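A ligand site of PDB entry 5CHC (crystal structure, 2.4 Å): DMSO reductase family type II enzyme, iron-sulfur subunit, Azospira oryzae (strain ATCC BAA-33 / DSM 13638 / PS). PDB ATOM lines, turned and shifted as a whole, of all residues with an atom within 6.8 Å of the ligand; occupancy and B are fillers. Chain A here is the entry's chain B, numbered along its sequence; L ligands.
SG of Cys 137 is bound to FE4 of the ligand (2.4 Å).
S4 of the ligand sits close to N of Ala 144.
An iron atom (FE2) of the ligand is bound by the side-chain sulfur (SG) of Cys 145, 2.4 Å away.
A sulfur (S2) of the ligand lies close to the backbone NH (N) of Asn 138, 3.3 Å away.
FE1 of the ligand is bound by SG of Cys 180, 2.4 Å away.
N of Cys 140 lies close to S1 of the ligand (3.7 Å).
An iron atom (FE3) of the ligand is bound by the side-chain sulfur of Cys 140, at 2.4 Å.
The backbone NH of Ala 183 sits close to the side-chain sulfur of Cys 180.
N of Lys 184 lies close to SG of Cys 180.
SG of Cys 137 lies close to N of His 139 (3.3 Å).
The side-chain sulfur of Cys 137 lies close to the side-chain amino group of Lys 196, at 3.1 Å.
The side-chain sulfur of Cys 180 sits close to the backbone NH of Tyr 182, at 3.1 Å.
The side-chain amino group (NZ) of Lys 196 sits at hydrogen-bond distance from the backbone carbonyl oxygen (O) of Val 163, 2.9 Å away.
The side-chain sulfur of Cys 140 lies close to the side-chain hydroxyl of Thr 252.
Residues that only touch the ligand: Pro 143, Tyr 182, Pro 185 and Lys 196.
Hydrophobic or aromatic side chains that line the ligand: Pro 143, Tyr 182 and Pro 185.
Ten residues have an atom within 4 Å of the ligand: Cys 137, Asn 138, Cys 140, Pro 143, Ala 144, Cys 145, Cys 180, Tyr 182, Pro 185 and Lys 196.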
ATOM      1  N   MET A 136      26.406  22.443  -1.548  1.00  0.00           N
ATOM      2  CA  MET A 136      25.616  21.790  -0.504  1.00  0.00           C
ATOM      3  C   MET A 136      24.352  21.321  -1.191  1.00  0.00           C
ATOM      4  O   MET A 136      24.219  21.438  -2.419  1.00  0.00           O
ATOM      5  CB  MET A 136      25.312  22.774   0.616  1.00  0.00           C
ATOM      6  CG  MET A 136      25.054  24.169   0.036  1.00  0.00           C
ATOM      7  SD  MET A 136      24.699  25.414   1.266  1.00  0.00           S
ATOM      8  CE  MET A 136      23.725  24.427   2.393  1.00  0.00           C
ATOM      9  N   CYS A 137      23.404  20.802  -0.418  1.00  0.00           N
ATOM     10  CA  CYS A 137      22.077  20.564  -0.974  1.00  0.00           C
ATOM     11  C   CYS A 137      21.420  21.933  -1.194  1.00  0.00           C
ATOM     12  O   CYS A 137      21.619  22.880  -0.418  1.00  0.00           O
ATOM     13  CB  CYS A 137      21.248  19.677  -0.040  1.00  0.00           C
ATOM     14  SG  CYS A 137      19.462  19.794  -0.285  1.00  0.00           S
ATOM     15  N   ASN A 138      20.653  22.063  -2.266  1.00  0.00           N
ATOM     16  CA  ASN A 138      20.127  23.385  -2.610  1.00  0.00           C
ATOM     17  C   ASN A 138      18.715  23.670  -2.088  1.00  0.00           C
ATOM     18  O   ASN A 138      18.140  24.740  -2.353  1.00  0.00           O
ATOM     19  CB  ASN A 138      20.174  23.556  -4.122  1.00  0.00           C
ATOM     20  CG  ASN A 138      21.595  23.590  -4.634  1.00  0.00           C
ATOM     21  OD1 ASN A 138      22.370  24.475  -4.250  1.00  0.00           O
ATOM     22  ND2 ASN A 138      21.961  22.641  -5.485  1.00  0.00           N
ATOM     23  N   HIS A 139      18.190  22.705  -1.336  1.00  0.00           N
ATOM     24  CA  HIS A 139      16.853  22.743  -0.761  1.00  0.00           C
ATOM     25  C   HIS A 139      15.897  23.389  -1.712  1.00  0.00           C
ATOM     26  O   HIS A 139      15.170  24.347  -1.396  1.00  0.00           O
ATOM     27  CB  HIS A 139      16.879  23.439   0.580  1.00  0.00           C
ATOM     28  CG  HIS A 139      17.808  22.758   1.536  1.00  0.00           C
ATOM     29  ND1 HIS A 139      17.440  21.640   2.255  1.00  0.00           N
ATOM     30  CD2 HIS A 139      19.108  22.990   1.832  1.00  0.00           C
ATOM     31  CE1 HIS A 139      18.458  21.230   2.986  1.00  0.00           C
ATOM     32  NE2 HIS A 139      19.489  22.033   2.742  1.00  0.00           N
ATOM     33  N   CYS A 140      15.953  22.835  -2.923  1.00  0.00           N
ATOM     34  CA  CYS A 140      15.230  23.266  -4.088  1.00  0.00           C
ATOM     35  C   CYS A 140      13.757  23.494  -3.855  1.00  0.00           C
ATOM     36  O   CYS A 140      13.109  22.788  -3.078  1.00  0.00           O
ATOM     37  CB  CYS A 140      15.442  22.240  -5.192  1.00  0.00           C
ATOM     38  SG  CYS A 140      17.171  22.098  -5.698  1.00  0.00           S
ATOM     39  N   THR A 141      13.230  24.485  -4.551  1.00  0.00           N
ATOM     40  CA  THR A 141      11.793  24.739  -4.561  1.00  0.00           C
ATOM     41  C   THR A 141      11.083  23.645  -5.381  1.00  0.00           C
ATOM     42  O   THR A 141       9.912  23.359  -5.149  1.00  0.00           O
ATOM     43  CB  THR A 141      11.511  26.155  -5.108  1.00  0.00           C
ATOM     44  OG1 THR A 141      11.928  27.123  -4.118  1.00  0.00           O
ATOM     45  CG2 THR A 141      10.031  26.341  -5.431  1.00  0.00           C
ATOM     46  N   LYS A 142      11.813  23.055  -6.335  1.00  0.00           N
ATOM     47  CA  LYS A 142      11.344  21.923  -7.118  1.00  0.00           C
ATOM     48  C   LYS A 142      12.283  20.714  -6.948  1.00  0.00           C
ATOM     49  O   LYS A 142      12.954  20.300  -7.892  1.00  0.00           O
ATOM     50  CB  LYS A 142      11.250  22.298  -8.608  1.00  0.00           C
ATOM     51  CG  LYS A 142      10.023  23.134  -9.028  1.00  0.00           C
ATOM     52  CD  LYS A 142       9.784  23.003 -10.554  1.00  0.00           C
ATOM     53  CE  LYS A 142       9.538  21.514 -10.966  1.00  0.00           C
ATOM     54  NZ  LYS A 142       8.984  21.269 -12.361  1.00  0.00           N
ATOM     55  N   PRO A 143      12.313  20.128  -5.746  1.00  0.00           N
ATOM     56  CA  PRO A 143      13.307  19.084  -5.477  1.00  0.00           C
ATOM     57  C   PRO A 143      13.109  17.802  -6.322  1.00  0.00           C
ATOM     58  O   PRO A 143      12.135  17.071  -6.139  1.00  0.00           O
ATOM     59  CB  PRO A 143      13.117  18.797  -3.980  1.00  0.00           C
ATOM     60  CG  PRO A 143      11.750  19.202  -3.685  1.00  0.00           C
ATOM     61  CD  PRO A 143      11.448  20.377  -4.577  1.00  0.00           C
ATOM     62  N   ALA A 144      14.036  17.563  -7.241  1.00  0.00           N
ATOM     63  CA  ALA A 144      13.996  16.360  -8.063  1.00  0.00           C
ATOM     64  C   ALA A 144      14.050  15.101  -7.211  1.00  0.00           C
ATOM     65  O   ALA A 144      13.335  14.150  -7.466  1.00  0.00           O
ATOM     66  CB  ALA A 144      15.146  16.360  -9.068  1.00  0.00           C
ATOM     67  N   CYS A 145      14.913  15.120  -6.205  1.00  0.00           N
ATOM     68  CA  CYS A 145      15.108  13.963  -5.358  1.00  0.00           C
ATOM     69  C   CYS A 145      13.780  13.504  -4.772  1.00  0.00           C
ATOM     70  O   CYS A 145      13.494  12.286  -4.692  1.00  0.00           O
ATOM     71  CB  CYS A 145      16.054  14.306  -4.236  1.00  0.00           C
ATOM     72  SG  CYS A 145      15.322  15.577  -3.221  1.00  0.00           S
ATOM     73  N   LEU A 146      12.998  14.485  -4.360  1.00  0.00           N
ATOM     74  CA  LEU A 146      11.800  14.246  -3.572  1.00  0.00           C
ATOM     75  C   LEU A 146      10.731  13.609  -4.447  1.00  0.00           C
ATOM     76  O   LEU A 146      10.096  12.667  -4.015  1.00  0.00           O
ATOM     77  CB  LEU A 146      11.305  15.554  -2.948  1.00  0.00           C
ATOM     78  CG  LEU A 146      10.043  15.571  -2.075  1.00  0.00           C
ATOM     79  CD1 LEU A 146      10.127  16.731  -1.088  1.00  0.00           C
ATOM     80  CD2 LEU A 146       8.771  15.680  -2.935  1.00  0.00           C
ATOM     81  N   ILE A 154      11.422  11.331   1.291  1.00  0.00           N
ATOM     82  CA  ILE A 154      11.952  12.686   1.267  1.00  0.00           C
ATOM     83  C   ILE A 154      10.828  13.713   1.337  1.00  0.00           C
ATOM     84  O   ILE A 154       9.914  13.692   0.536  1.00  0.00           O
ATOM     85  CB  ILE A 154      12.820  12.927   0.017  1.00  0.00           C
ATOM     86  CG1 ILE A 154      13.896  11.849  -0.074  1.00  0.00           C
ATOM     87  CG2 ILE A 154      13.510  14.299   0.084  1.00  0.00           C
ATOM     88  CD1 ILE A 154      14.896  12.100  -1.167  1.00  0.00           C
ATOM     89  N   VAL A 163      14.634  20.605   2.936  1.00  0.00           N
ATOM     90  CA  VAL A 163      14.386  19.248   2.450  1.00  0.00           C
ATOM     91  C   VAL A 163      15.169  18.185   3.222  1.00  0.00           C
ATOM     92  O   VAL A 163      16.368  18.334   3.482  1.00  0.00           O
ATOM     93  CB  VAL A 163      14.715  19.149   0.953  1.00  0.00           C
ATOM     94  CG1 VAL A 163      14.478  17.752   0.453  1.00  0.00           C
ATOM     95  CG2 VAL A 163      13.856  20.138   0.163  1.00  0.00           C
ATOM     96  N   CYS A 176      16.647   8.905  -5.788  1.00  0.00           N
ATOM     97  CA  CYS A 176      17.023  10.268  -5.483  1.00  0.00           C
ATOM     98  C   CYS A 176      18.453  10.579  -5.994  1.00  0.00           C
ATOM     99  O   CYS A 176      18.691  11.646  -6.560  1.00  0.00           O
ATOM    100  CB  CYS A 176      16.910  10.504  -3.982  1.00  0.00           C
ATOM    101  SG  CYS A 176      18.008   9.474  -3.008  1.00  0.00           S
ATOM    102  N   SER A 179      18.373  11.163  -9.618  1.00  0.00           N
ATOM    103  CA  SER A 179      17.609  12.347 -10.036  1.00  0.00           C
ATOM    104  C   SER A 179      18.121  13.709  -9.583  1.00  0.00           C
ATOM    105  O   SER A 179      17.800  14.732 -10.207  1.00  0.00           O
ATOM    106  CB  SER A 179      16.159  12.200  -9.566  1.00  0.00           C
ATOM    107  OG  SER A 179      15.429  11.446 -10.504  1.00  0.00           O
ATOM    108  N   CYS A 180      18.864  13.763  -8.481  1.00  0.00           N
ATOM    109  CA  CYS A 180      19.523  15.004  -8.120  1.00  0.00           C
ATOM    110  C   CYS A 180      20.675  15.296  -9.073  1.00  0.00           C
ATOM    111  O   CYS A 180      21.666  14.560  -9.103  1.00  0.00           O
ATOM    112  CB  CYS A 180      20.045  14.983  -6.692  1.00  0.00           C
ATOM    113  SG  CYS A 180      21.100  16.397  -6.419  1.00  0.00           S
ATOM    114  N   PRO A 181      20.549  16.394  -9.830  1.00  0.00           N
ATOM    115  CA  PRO A 181      21.592  16.729 -10.801  1.00  0.00           C
ATOM    116  C   PRO A 181      22.816  17.355 -10.118  1.00  0.00           C
ATOM    117  O   PRO A 181      23.817  17.609 -10.790  1.00  0.00           O
ATOM    118  CB  PRO A 181      20.893  17.737 -11.710  1.00  0.00           C
ATOM    119  CG  PRO A 181      19.939  18.454 -10.763  1.00  0.00           C
ATOM    120  CD  PRO A 181      19.496  17.423  -9.749  1.00  0.00           C
ATOM    121  N   TYR A 182      22.735  17.612  -8.808  1.00  0.00           N
ATOM    122  CA  TYR A 182      23.850  18.190  -8.050  1.00  0.00           C
ATOM    123  C   TYR A 182      24.655  17.102  -7.333  1.00  0.00           C
ATOM    124  O   TYR A 182      25.633  17.381  -6.668  1.00  0.00           O
ATOM    125  CB  TYR A 182      23.323  19.223  -7.068  1.00  0.00           C
ATOM    126  CG  TYR A 182      22.643  20.386  -7.752  1.00  0.00           C
ATOM    127  CD1 TYR A 182      23.376  21.458  -8.237  1.00  0.00           C
ATOM    128  CD2 TYR A 182      21.265  20.400  -7.945  1.00  0.00           C
ATOM    129  CE1 TYR A 182      22.778  22.507  -8.876  1.00  0.00           C
ATOM    130  CE2 TYR A 182      20.635  21.454  -8.584  1.00  0.00           C
ATOM    131  CZ  TYR A 182      21.400  22.503  -9.057  1.00  0.00           C
ATOM    132  OH  TYR A 182      20.790  23.551  -9.689  1.00  0.00           O
ATOM    133  N   ALA A 183      24.200  15.848  -7.482  1.00  0.00           N
ATOM    134  CA  ALA A 183      24.776  14.702  -6.779  1.00  0.00           C
ATOM    135  C   ALA A 183      24.942  14.930  -5.283  1.00  0.00           C
ATOM    136  O   ALA A 183      26.007  14.616  -4.734  1.00  0.00           O
ATOM    137  CB  ALA A 183      26.116  14.323  -7.390  1.00  0.00           C
ATOM    138  N   LYS A 184      23.905  15.452  -4.642  1.00  0.00           N
ATOM    139  CA  LYS A 184      23.992  15.751  -3.209  1.00  0.00           C
ATOM    140  C   LYS A 184      23.322  14.751  -2.236  1.00  0.00           C
ATOM    141  O   LYS A 184      23.599  14.815  -1.040  1.00  0.00           O
ATOM    142  CB  LYS A 184      23.441  17.156  -2.957  1.00  0.00           C
ATOM    143  CG  LYS A 184      24.543  18.250  -3.096  1.00  0.00           C
ATOM    144  CD  LYS A 184      25.648  18.034  -2.069  1.00  0.00           C
ATOM    145  CE  LYS A 184      26.953  18.730  -2.449  1.00  0.00           C
ATOM    146  NZ  LYS A 184      28.074  18.316  -1.559  1.00  0.00           N
ATOM    147  N   PRO A 185      22.459  13.819  -2.718  1.00  0.00           N
ATOM    148  CA  PRO A 185      22.150  12.681  -1.832  1.00  0.00           C
ATOM    149  C   PRO A 185      23.199  11.546  -1.938  1.00  0.00           C
ATOM    150  O   PRO A 185      23.587  11.209  -3.051  1.00  0.00           O
ATOM    151  CB  PRO A 185      20.783  12.188  -2.339  1.00  0.00           C
ATOM    152  CG  PRO A 185      20.350  13.138  -3.391  1.00  0.00           C
ATOM    153  CD  PRO A 185      21.585  13.806  -3.907  1.00  0.00           C
ATOM    154  N   LYS A 196      21.914  12.995   3.294  1.00  0.00           N
ATOM    155  CA  LYS A 196      22.247  14.304   2.749  1.00  0.00           C
ATOM    156  C   LYS A 196      22.057  15.432   3.746  1.00  0.00           C
ATOM    157  O   LYS A 196      21.460  15.263   4.823  1.00  0.00           O
ATOM    158  CB  LYS A 196      21.425  14.607   1.499  1.00  0.00           C
ATOM    159  CG  LYS A 196      20.076  15.189   1.796  1.00  0.00           C
ATOM    160  CD  LYS A 196      19.420  15.667   0.521  1.00  0.00           C
ATOM    161  CE  LYS A 196      18.180  16.487   0.866  1.00  0.00           C
ATOM    162  NZ  LYS A 196      18.533  17.662   1.725  1.00  0.00           N
ATOM    163  N   CYS A 197      22.626  16.575   3.372  1.00  0.00           N
ATOM    164  CA  CYS A 197      22.506  17.842   4.086  1.00  0.00           C
ATOM    165  C   CYS A 197      21.122  18.070   4.694  1.00  0.00           C
ATOM    166  O   CYS A 197      20.112  17.945   3.997  1.00  0.00           O
ATOM    167  CB  CYS A 197      22.868  18.966   3.102  1.00  0.00           C
ATOM    168  SG  CYS A 197      22.227  20.606   3.464  1.00  0.00           S
ATOM    169  N   THR A 252      15.508  22.797 -11.029  1.00  0.00           N
ATOM    170  CA  THR A 252      15.084  22.433  -9.693  1.00  0.00           C
ATOM    171  C   THR A 252      14.784  23.685  -8.867  1.00  0.00           C
ATOM    172  O   THR A 252      14.258  23.583  -7.752  1.00  0.00           O
ATOM    173  CB  THR A 252      16.164  21.571  -8.980  1.00  0.00           C
ATOM    174  OG1 THR A 252      17.285  22.382  -8.639  1.00  0.00           O
ATOM    175  CG2 THR A 252      16.623  20.436  -9.881  1.00  0.00           C
ATOM    176  N   PRO A 254      17.001  26.080  -7.296  1.00  0.00           N
ATOM    177  CA  PRO A 254      17.750  26.083  -6.041  1.00  0.00           C
ATOM    178  C   PRO A 254      17.380  27.243  -5.135  1.00  0.00           C
ATOM    179  O   PRO A 254      16.862  28.253  -5.619  1.00  0.00           O
ATOM    180  CB  PRO A 254      19.215  26.225  -6.485  1.00  0.00           C
ATOM    181  CG  PRO A 254      19.241  25.724  -7.878  1.00  0.00           C
ATOM    182  CD  PRO A 254      17.899  26.060  -8.473  1.00  0.00           C
HETATM  183 FE1  LIG L   1      19.487  17.607  -5.119  1.00  0.00          FE
HETATM  184 FE2  LIG L   1      17.006  17.259  -3.770  1.00  0.00          FE
HETATM  185 FE3  LIG L   1      17.722  19.900  -4.899  1.00  0.00          FE
HETATM  186 FE4  LIG L   1      19.073  18.905  -2.451  1.00  0.00          FE
HETATM  187  S1  LIG L   1      16.950  19.261  -2.968  1.00  0.00           S
HETATM  188  S2  LIG L   1      19.844  19.595  -4.376  1.00  0.00           S
HETATM  189  S3  LIG L   1      19.072  16.852  -3.098  1.00  0.00           S
HETATM  190  S4  LIG L   1      17.435  17.945  -5.792  1.00  0.00           S
